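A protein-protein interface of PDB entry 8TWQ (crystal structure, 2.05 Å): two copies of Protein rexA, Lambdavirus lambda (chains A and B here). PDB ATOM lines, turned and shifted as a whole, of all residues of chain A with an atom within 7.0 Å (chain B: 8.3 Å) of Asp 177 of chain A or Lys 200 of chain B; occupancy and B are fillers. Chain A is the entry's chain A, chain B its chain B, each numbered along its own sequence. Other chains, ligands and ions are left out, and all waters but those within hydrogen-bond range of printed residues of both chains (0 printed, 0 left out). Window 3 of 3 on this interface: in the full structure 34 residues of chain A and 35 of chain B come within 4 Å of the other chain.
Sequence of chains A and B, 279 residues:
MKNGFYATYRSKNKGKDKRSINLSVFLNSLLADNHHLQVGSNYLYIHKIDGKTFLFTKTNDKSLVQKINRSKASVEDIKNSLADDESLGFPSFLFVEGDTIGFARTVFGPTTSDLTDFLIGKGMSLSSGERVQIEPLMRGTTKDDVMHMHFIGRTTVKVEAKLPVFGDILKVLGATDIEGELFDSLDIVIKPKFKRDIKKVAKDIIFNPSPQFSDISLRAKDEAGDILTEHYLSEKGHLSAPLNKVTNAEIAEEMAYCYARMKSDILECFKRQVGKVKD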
ATOM      1  N   LYS A 171     -20.024 -10.334  -5.863  1.00  0.00           N
ATOM      2  CA  LYS A 171     -21.216 -11.129  -6.165  1.00  0.00           C
ATOM      3  C   LYS A 171     -21.055 -11.904  -7.466  1.00  0.00           C
ATOM      4  O   LYS A 171     -21.499 -13.058  -7.566  1.00  0.00           O
ATOM      5  CB  LYS A 171     -22.453 -10.231  -6.236  1.00  0.00           C
ATOM      6  CG  LYS A 171     -23.117 -10.000  -4.882  1.00  0.00           C
ATOM      7  CD  LYS A 171     -24.598 -10.392  -4.887  1.00  0.00           C
ATOM      8  CE  LYS A 171     -25.166 -10.519  -3.460  1.00  0.00           C
ATOM      9  NZ  LYS A 171     -26.189 -11.615  -3.318  1.00  0.00           N
ATOM     10  N   GLY A 174     -19.529 -14.892  -6.782  1.00  0.00           N
ATOM     11  CA  GLY A 174     -20.412 -15.760  -6.032  1.00  0.00           C
ATOM     12  C   GLY A 174     -20.582 -15.412  -4.572  1.00  0.00           C
ATOM     13  O   GLY A 174     -21.098 -16.240  -3.817  1.00  0.00           O
ATOM     14  N   ALA A 175     -20.151 -14.234  -4.140  1.00  0.00           N
ATOM     15  CA  ALA A 175     -20.250 -13.857  -2.736  1.00  0.00           C
ATOM     16  C   ALA A 175     -21.560 -13.105  -2.541  1.00  0.00           C
ATOM     17  O   ALA A 175     -21.730 -11.996  -3.050  1.00  0.00           O
ATOM     18  CB  ALA A 175     -19.048 -13.017  -2.320  1.00  0.00           C
ATOM     19  N   THR A 176     -22.484 -13.709  -1.797  1.00  0.00           N
ATOM     20  CA  THR A 176     -23.820 -13.155  -1.601  1.00  0.00           C
ATOM     21  C   THR A 176     -24.047 -12.663  -0.177  1.00  0.00           C
ATOM     22  O   THR A 176     -25.199 -12.519   0.254  1.00  0.00           O
ATOM     23  CB  THR A 176     -24.869 -14.203  -1.957  1.00  0.00           C
ATOM     24  OG1 THR A 176     -24.556 -15.423  -1.263  1.00  0.00           O
ATOM     25  CG2 THR A 176     -24.884 -14.435  -3.474  1.00  0.00           C
ATOM     26  N   ASP A 177     -22.969 -12.416   0.572  1.00  0.00           N
ATOM     27  CA  ASP A 177     -23.113 -12.026   1.969  1.00  0.00           C
ATOM     28  C   ASP A 177     -21.870 -11.216   2.333  1.00  0.00           C
ATOM     29  O   ASP A 177     -20.935 -11.702   2.985  1.00  0.00           O
ATOM     30  CB  ASP A 177     -23.293 -13.241   2.880  1.00  0.00           C
ATOM     31  CG  ASP A 177     -23.404 -12.863   4.339  1.00  0.00           C
ATOM     32  OD1 ASP A 177     -24.243 -11.988   4.657  1.00  0.00           O
ATOM     33  OD2 ASP A 177     -22.655 -13.445   5.162  1.00  0.00           O
ATOM     34  N   ILE A 178     -21.862  -9.959   1.900  1.00  0.00           N
ATOM     35  CA  ILE A 178     -20.693  -9.103   2.036  1.00  0.00           C
ATOM     36  C   ILE A 178     -20.946  -8.096   3.152  1.00  0.00           C
ATOM     37  O   ILE A 178     -21.893  -7.306   3.078  1.00  0.00           O
ATOM     38  CB  ILE A 178     -20.361  -8.401   0.712  1.00  0.00           C
ATOM     39  CG1 ILE A 178     -20.340  -9.421  -0.426  1.00  0.00           C
ATOM     40  CG2 ILE A 178     -19.014  -7.703   0.808  1.00  0.00           C
ATOM     41  CD1 ILE A 178     -20.871  -8.886  -1.736  1.00  0.00           C
ATOM     42  N   GLU A 179     -20.106  -8.141   4.193  1.00  0.00           N
ATOM     43  CA  GLU A 179     -20.067  -7.139   5.264  1.00  0.00           C
ATOM     44  C   GLU A 179     -18.911  -6.193   4.967  1.00  0.00           C
ATOM     45  O   GLU A 179     -17.817  -6.326   5.515  1.00  0.00           O
ATOM     46  CB  GLU A 179     -19.876  -7.812   6.620  1.00  0.00           C
ATOM     47  CG  GLU A 179     -21.113  -8.539   7.171  1.00  0.00           C
ATOM     48  CD  GLU A 179     -21.043 -10.053   7.035  1.00  0.00           C
ATOM     49  OE1 GLU A 179     -19.917 -10.595   6.919  1.00  0.00           O
ATOM     50  OE2 GLU A 179     -22.120 -10.704   7.050  1.00  0.00           O
ATOM     51  N   GLY A 180     -19.155  -5.232   4.075  1.00  0.00           N
ATOM     52  CA  GLY A 180     -18.107  -4.356   3.563  1.00  0.00           C
ATOM     53  C   GLY A 180     -17.183  -3.724   4.590  1.00  0.00           C
ATOM     54  O   GLY A 180     -16.070  -3.288   4.265  1.00  0.00           O
ATOM     55  N   LEU A 182     -15.716  -5.316   6.937  1.00  0.00           N
ATOM     56  CA  LEU A 182     -14.599  -6.228   7.148  1.00  0.00           C
ATOM     57  C   LEU A 182     -13.440  -5.966   6.204  1.00  0.00           C
ATOM     58  O   LEU A 182     -12.330  -6.451   6.451  1.00  0.00           O
ATOM     59  CB  LEU A 182     -15.051  -7.668   6.969  1.00  0.00           C
ATOM     60  CG  LEU A 182     -16.046  -8.122   8.015  1.00  0.00           C
ATOM     61  CD1 LEU A 182     -16.266  -9.602   7.865  1.00  0.00           C
ATOM     62  CD2 LEU A 182     -15.571  -7.753   9.436  1.00  0.00           C
ATOM     63  N   PHE A 183     -13.660  -5.212   5.145  1.00  0.00           N
ATOM     64  CA  PHE A 183     -12.776  -5.241   4.000  1.00  0.00           C
ATOM     65  C   PHE A 183     -12.093  -3.901   3.836  1.00  0.00           C
ATOM     66  O   PHE A 183     -12.634  -2.857   4.211  1.00  0.00           O
ATOM     67  CB  PHE A 183     -13.556  -5.586   2.726  1.00  0.00           C
ATOM     68  CG  PHE A 183     -14.112  -6.980   2.718  1.00  0.00           C
ATOM     69  CD1 PHE A 183     -13.359  -8.040   2.226  1.00  0.00           C
ATOM     70  CD2 PHE A 183     -15.380  -7.236   3.206  1.00  0.00           C
ATOM     71  CE1 PHE A 183     -13.870  -9.312   2.215  1.00  0.00           C
ATOM     72  CE2 PHE A 183     -15.890  -8.517   3.200  1.00  0.00           C
ATOM     73  CZ  PHE A 183     -15.136  -9.555   2.711  1.00  0.00           C
ATOM     74  N   MET B 147     -13.427 -25.252   4.254  1.00  0.00           N
ATOM     75  CA  MET B 147     -14.639 -25.040   5.019  1.00  0.00           C
ATOM     76  C   MET B 147     -14.427 -25.174   6.513  1.00  0.00           C
ATOM     77  O   MET B 147     -15.240 -24.683   7.295  1.00  0.00           O
ATOM     78  CB  MET B 147     -15.721 -26.012   4.578  1.00  0.00           C
ATOM     79  CG  MET B 147     -16.102 -25.849   3.126  1.00  0.00           C
ATOM     80  SD  MET B 147     -17.265 -24.296   2.796  1.00  0.00           S
ATOM     81  CE  MET B 147     -16.037 -23.262   1.791  1.00  0.00           C
ATOM     82  N   MET B 149     -11.520 -24.110   7.949  1.00  0.00           N
ATOM     83  CA  MET B 149     -10.507 -23.132   8.346  1.00  0.00           C
ATOM     84  C   MET B 149     -11.006 -22.173   9.409  1.00  0.00           C
ATOM     85  O   MET B 149     -12.105 -21.617   9.310  1.00  0.00           O
ATOM     86  CB  MET B 149     -10.005 -22.335   7.149  1.00  0.00           C
ATOM     87  CG  MET B 149      -8.760 -22.914   6.562  1.00  0.00           C
ATOM     88  SD  MET B 149      -8.366 -22.323   4.769  1.00  0.00           S
ATOM     89  CE  MET B 149      -8.459 -20.488   4.908  1.00  0.00           C
ATOM     90  N   PHE B 151      -9.519 -19.213  10.467  1.00  0.00           N
ATOM     91  CA  PHE B 151      -9.371 -17.817  10.080  1.00  0.00           C
ATOM     92  C   PHE B 151      -8.929 -17.738   8.630  1.00  0.00           C
ATOM     93  O   PHE B 151      -8.021 -18.469   8.223  1.00  0.00           O
ATOM     94  CB  PHE B 151      -8.332 -17.106  10.958  1.00  0.00           C
ATOM     95  CG  PHE B 151      -8.036 -15.696  10.533  1.00  0.00           C
ATOM     96  CD1 PHE B 151      -8.782 -14.637  11.043  1.00  0.00           C
ATOM     97  CD2 PHE B 151      -7.002 -15.416   9.632  1.00  0.00           C
ATOM     98  CE1 PHE B 151      -8.520 -13.348  10.656  1.00  0.00           C
ATOM     99  CE2 PHE B 151      -6.735 -14.124   9.240  1.00  0.00           C
ATOM    100  CZ  PHE B 151      -7.494 -13.084   9.760  1.00  0.00           C
ATOM    101  N   ILE B 152      -9.528 -16.827   7.859  1.00  0.00           N
ATOM    102  CA  ILE B 152      -9.095 -16.582   6.487  1.00  0.00           C
ATOM    103  C   ILE B 152      -8.892 -15.091   6.282  1.00  0.00           C
ATOM    104  O   ILE B 152      -9.826 -14.302   6.468  1.00  0.00           O
ATOM    105  CB  ILE B 152     -10.096 -17.106   5.440  1.00  0.00           C
ATOM    106  CG1 ILE B 152     -10.458 -18.562   5.704  1.00  0.00           C
ATOM    107  CG2 ILE B 152      -9.516 -16.931   4.038  1.00  0.00           C
ATOM    108  CD1 ILE B 152     -11.492 -19.089   4.730  1.00  0.00           C
ATOM    109  N   THR B 155      -7.406 -13.130   0.316  1.00  0.00           N
ATOM    110  CA  THR B 155      -7.804 -14.176  -0.612  1.00  0.00           C
ATOM    111  C   THR B 155      -7.612 -13.655  -2.025  1.00  0.00           C
ATOM    112  O   THR B 155      -8.036 -12.542  -2.338  1.00  0.00           O
ATOM    113  CB  THR B 155      -9.254 -14.581  -0.364  1.00  0.00           C
ATOM    114  OG1 THR B 155      -9.369 -15.094   0.973  1.00  0.00           O
ATOM    115  CG2 THR B 155      -9.742 -15.626  -1.403  1.00  0.00           C
ATOM    116  N   ASP B 197     -11.460 -11.302   9.787  1.00  0.00           N
ATOM    117  CA  ASP B 197     -11.711 -12.611   9.195  1.00  0.00           C
ATOM    118  C   ASP B 197     -12.698 -12.456   8.049  1.00  0.00           C
ATOM    119  O   ASP B 197     -13.865 -12.126   8.276  1.00  0.00           O
ATOM    120  CB  ASP B 197     -12.260 -13.571  10.240  1.00  0.00           C
ATOM    121  CG  ASP B 197     -12.223 -15.016   9.783  1.00  0.00           C
ATOM    122  OD1 ASP B 197     -11.853 -15.288   8.631  1.00  0.00           O
ATOM    123  OD2 ASP B 197     -12.547 -15.900  10.589  1.00  0.00           O
ATOM    124  N   ILE B 198     -12.239 -12.687   6.818  1.00  0.00           N
ATOM    125  CA  ILE B 198     -13.136 -12.590   5.670  1.00  0.00           C
ATOM    126  C   ILE B 198     -13.475 -13.984   5.149  1.00  0.00           C
ATOM    127  O   ILE B 198     -13.664 -14.185   3.943  1.00  0.00           O
ATOM    128  CB  ILE B 198     -12.536 -11.696   4.569  1.00  0.00           C
ATOM    129  CG1 ILE B 198     -11.201 -12.235   4.064  1.00  0.00           C
ATOM    130  CG2 ILE B 198     -12.355 -10.273   5.076  1.00  0.00           C
ATOM    131  CD1 ILE B 198     -10.736 -11.537   2.805  1.00  0.00           C
ATOM    132  N   LYS B 199     -13.608 -14.950   6.060  1.00  0.00           N
ATOM    133  CA  LYS B 199     -13.820 -16.321   5.628  1.00  0.00           C
ATOM    134  C   LYS B 199     -15.205 -16.566   5.048  1.00  0.00           C
ATOM    135  O   LYS B 199     -15.381 -17.539   4.320  1.00  0.00           O
ATOM    136  CB  LYS B 199     -13.563 -17.290   6.780  1.00  0.00           C
ATOM    137  CG  LYS B 199     -14.606 -17.364   7.865  1.00  0.00           C
ATOM    138  CD  LYS B 199     -13.995 -18.066   9.073  1.00  0.00           C
ATOM    139  CE  LYS B 199     -14.915 -19.068   9.716  1.00  0.00           C
ATOM    140  NZ  LYS B 199     -14.296 -19.577  10.970  1.00  0.00           N
ATOM    141  N   LYS B 200     -16.190 -15.712   5.318  1.00  0.00           N
ATOM    142  CA  LYS B 200     -17.517 -15.973   4.777  1.00  0.00           C
ATOM    143  C   LYS B 200     -17.558 -15.675   3.283  1.00  0.00           C
ATOM    144  O   LYS B 200     -18.036 -16.493   2.487  1.00  0.00           O
ATOM    145  CB  LYS B 200     -18.563 -15.168   5.549  1.00  0.00           C
ATOM    146  CG  LYS B 200     -19.888 -15.015   4.851  1.00  0.00           C
ATOM    147  CD  LYS B 200     -20.780 -16.258   4.960  1.00  0.00           C
ATOM    148  CE  LYS B 200     -21.793 -16.281   3.788  1.00  0.00           C
ATOM    149  NZ  LYS B 200     -22.996 -17.140   3.992  1.00  0.00           N
ATOM    150  N   VAL B 201     -17.027 -14.528   2.875  1.00  0.00           N
ATOM    151  CA  VAL B 201     -16.888 -14.258   1.451  1.00  0.00           C
ATOM    152  C   VAL B 201     -15.961 -15.288   0.803  1.00  0.00           C
ATOM    153  O   VAL B 201     -16.325 -15.942  -0.182  1.00  0.00           O
ATOM    154  CB  VAL B 201     -16.411 -12.813   1.230  1.00  0.00           C
ATOM    155  CG1 VAL B 201     -15.986 -12.587  -0.220  1.00  0.00           C
ATOM    156  CG2 VAL B 201     -17.526 -11.847   1.607  1.00  0.00           C
ATOM    157  N   ALA B 202     -14.770 -15.487   1.376  1.00  0.00           N
ATOM    158  CA  ALA B 202     -13.825 -16.469   0.837  1.00  0.00           C
ATOM    159  C   ALA B 202     -14.464 -17.854   0.648  1.00  0.00           C
ATOM    160  O   ALA B 202     -14.300 -18.488  -0.397  1.00  0.00           O
ATOM    161  CB  ALA B 202     -12.600 -16.555   1.750  1.00  0.00           C
ATOM    162  N   LYS B 203     -15.201 -18.341   1.648  1.00  0.00           N
ATOM    163  CA  LYS B 203     -15.885 -19.626   1.504  1.00  0.00           C
ATOM    164  C   LYS B 203     -16.948 -19.579   0.404  1.00  0.00           C
ATOM    165  O   LYS B 203     -17.126 -20.561  -0.321  1.00  0.00           O
ATOM    166  CB  LYS B 203     -16.522 -20.040   2.832  1.00  0.00           C
ATOM    167  CG  LYS B 203     -15.564 -20.557   3.919  1.00  0.00           C
ATOM    168  CD  LYS B 203     -16.251 -20.481   5.300  1.00  0.00           C
ATOM    169  CE  LYS B 203     -15.671 -21.482   6.304  1.00  0.00           C
ATOM    170  NZ  LYS B 203     -14.187 -21.351   6.515  1.00  0.00           N
ATOM    171  N   ASP B 204     -17.660 -18.446   0.260  1.00  0.00           N
ATOM    172  CA  ASP B 204     -18.765 -18.348  -0.704  1.00  0.00           C
ATOM    173  C   ASP B 204     -18.270 -18.457  -2.137  1.00  0.00           C
ATOM    174  O   ASP B 204     -18.917 -19.085  -2.982  1.00  0.00           O
ATOM    175  CB  ASP B 204     -19.516 -17.018  -0.541  1.00  0.00           C
ATOM    176  CG  ASP B 204     -20.696 -17.104   0.420  1.00  0.00           C
ATOM    177  OD1 ASP B 204     -20.917 -18.180   1.028  1.00  0.00           O
ATOM    178  OD2 ASP B 204     -21.391 -16.064   0.567  1.00  0.00           O
ATOM    179  N   ILE B 205     -17.132 -17.823  -2.429  1.00  0.00           N
ATOM    180  CA  ILE B 205     -16.525 -17.893  -3.753  1.00  0.00           C
ATOM    181  C   ILE B 205     -15.981 -19.294  -4.019  1.00  0.00           C
ATOM    182  O   ILE B 205     -16.182 -19.866  -5.103  1.00  0.00           O
ATOM    183  CB  ILE B 205     -15.439 -16.807  -3.847  1.00  0.00           C
ATOM    184  CG1 ILE B 205     -16.084 -15.423  -3.761  1.00  0.00           C
ATOM    185  CG2 ILE B 205     -14.554 -16.969  -5.088  1.00  0.00           C
ATOM    186  CD1 ILE B 205     -15.091 -14.313  -3.426  1.00  0.00           C
ATOM    187  N   ILE B 206     -15.316 -19.884  -3.023  1.00  0.00           N
ATOM    188  CA  ILE B 206     -14.612 -21.144  -3.241  1.00  0.00           C
ATOM    189  C   ILE B 206     -15.596 -22.285  -3.405  1.00  0.00           C
ATOM    190  O   ILE B 206     -15.321 -23.251  -4.132  1.00  0.00           O
ATOM    191  CB  ILE B 206     -13.630 -21.421  -2.087  1.00  0.00           C
ATOM    192  CG1 ILE B 206     -12.446 -20.454  -2.140  1.00  0.00           C
ATOM    193  CG2 ILE B 206     -13.147 -22.874  -2.096  1.00  0.00           C
ATOM    194  CD1 ILE B 206     -11.584 -20.474  -0.896  1.00  0.00           C
ATOM    195  N   PHE B 207     -16.744 -22.213  -2.734  1.00  0.00           N
ATOM    196  CA  PHE B 207     -17.725 -23.282  -2.801  1.00  0.00           C
ATOM    197  C   PHE B 207     -18.823 -23.014  -3.820  1.00  0.00           C
ATOM    198  O   PHE B 207     -19.785 -23.786  -3.896  1.00  0.00           O
ATOM    199  CB  PHE B 207     -18.315 -23.533  -1.420  1.00  0.00           C
ATOM    200  CG  PHE B 207     -17.850 -24.816  -0.817  1.00  0.00           C
ATOM    201  CD1 PHE B 207     -16.508 -24.974  -0.490  1.00  0.00           C
ATOM    202  CD2 PHE B 207     -18.711 -25.898  -0.665  1.00  0.00           C
ATOM    203  CE1 PHE B 207     -16.045 -26.149   0.045  1.00  0.00           C
ATOM    204  CE2 PHE B 207     -18.245 -27.112  -0.134  1.00  0.00           C
ATOM    205  CZ  PHE B 207     -16.907 -27.238   0.217  1.00  0.00           C
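The side-chain carboxylate (OD2) of Asp 177 of chain A is in salt-bridge range of the side-chain amino group (NZ) of Lys 200 of chain B, at 3.9 Å.
The backbone NH (N) of Ile 152 of chain B sits at hydrogen-bond distance from the side-chain carboxylate (OD1) of Asp 197 of chain B, 2.9 Å away.
The backbone carbonyl oxygen (O) of Ile 152 of chain B lies within hydrogen-bond range of the backbone NH (N) of Ile 198 of chain B (2.9 Å).
The side-chain carboxylate (OD1) of Asp 204 of chain B is in salt-bridge range of the side-chain amino group (NZ) of Lys 200 of chain B, at 3.8 Å.
OD1 of Asp 197 of chain B is in hydrogen-bond range of N of Lys 199 of chain B, 3.1 Å away.
Among the printed residues, pairs that only touch across the chains: Phe 183 of chain A with Ile 198 of chain B, Phe 183 of chain A with Val 201 of chain B, Leu 182 of chain A with Asp 197 of chain B, Thr 176 of chain A with Asp 204 of chain B, Asp 177 of chain A with Val 201 of chain B, Gly 174 of chain A with Asp 204 of chain B, Ala 175 of chain A with Val 201 of chain B, Ala 175 of chain A with Asp 204 of chain B and Asp 177 of chain A with Asp 204 of chain B.
Of the printed residues of chain B, Gly 174 of chain A touches Asp 204 (3.7 Å).
Printed residues of chain B within 4 Å of Thr 176 of chain A: Asp 204.
Asp 177 of chain A touches three residues of chain B.
Printed residues of chain B within 4 Å of Leu 182 of chain A: Asp 197.
Of the printed residues of chain B, Phe 183 of chain A touches Ile 198 (3.4 Å) and Val 201 (3.5 Å).
Of chain A, only Asp 177 (3.2 Å) comes within 4 Å of Lys 200 of chain B.
Of the printed residues of chain A, Val 201 of chain B touches Ala 175 (3.7 Å), Asp 177 (3.7 Å) and Phe 183 (3.5 Å).
Ala 202 of chain B touches none of the printed residues of chain A.
The nearest residue of chain B that does not touch Asp 177 of chain A is Ala 202 of chain B (7.4 Å).
Of the 16 printed residues of chain B, 5 touch a printed residue of chain A.
Printed residues of chain B that touch a printed residue of chain A: Asp 197, Ile 198, Lys 200, Val 201 and Asp 204.
Of the 10 printed residues of chain A, 6 touch a printed residue of chain B.
Hydrophobic or aromatic side chains of chain A that line the printed part of chain B: Ala 175, Leu 182 and Phe 183.
Among the printed residues, Asp or Glu carboxylates within 4 Å of a Lys or Arg side-chain nitrogen of the other chain: Asp 177 of chain A with Lys 200 of chain B.
No position is printed for both chains.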
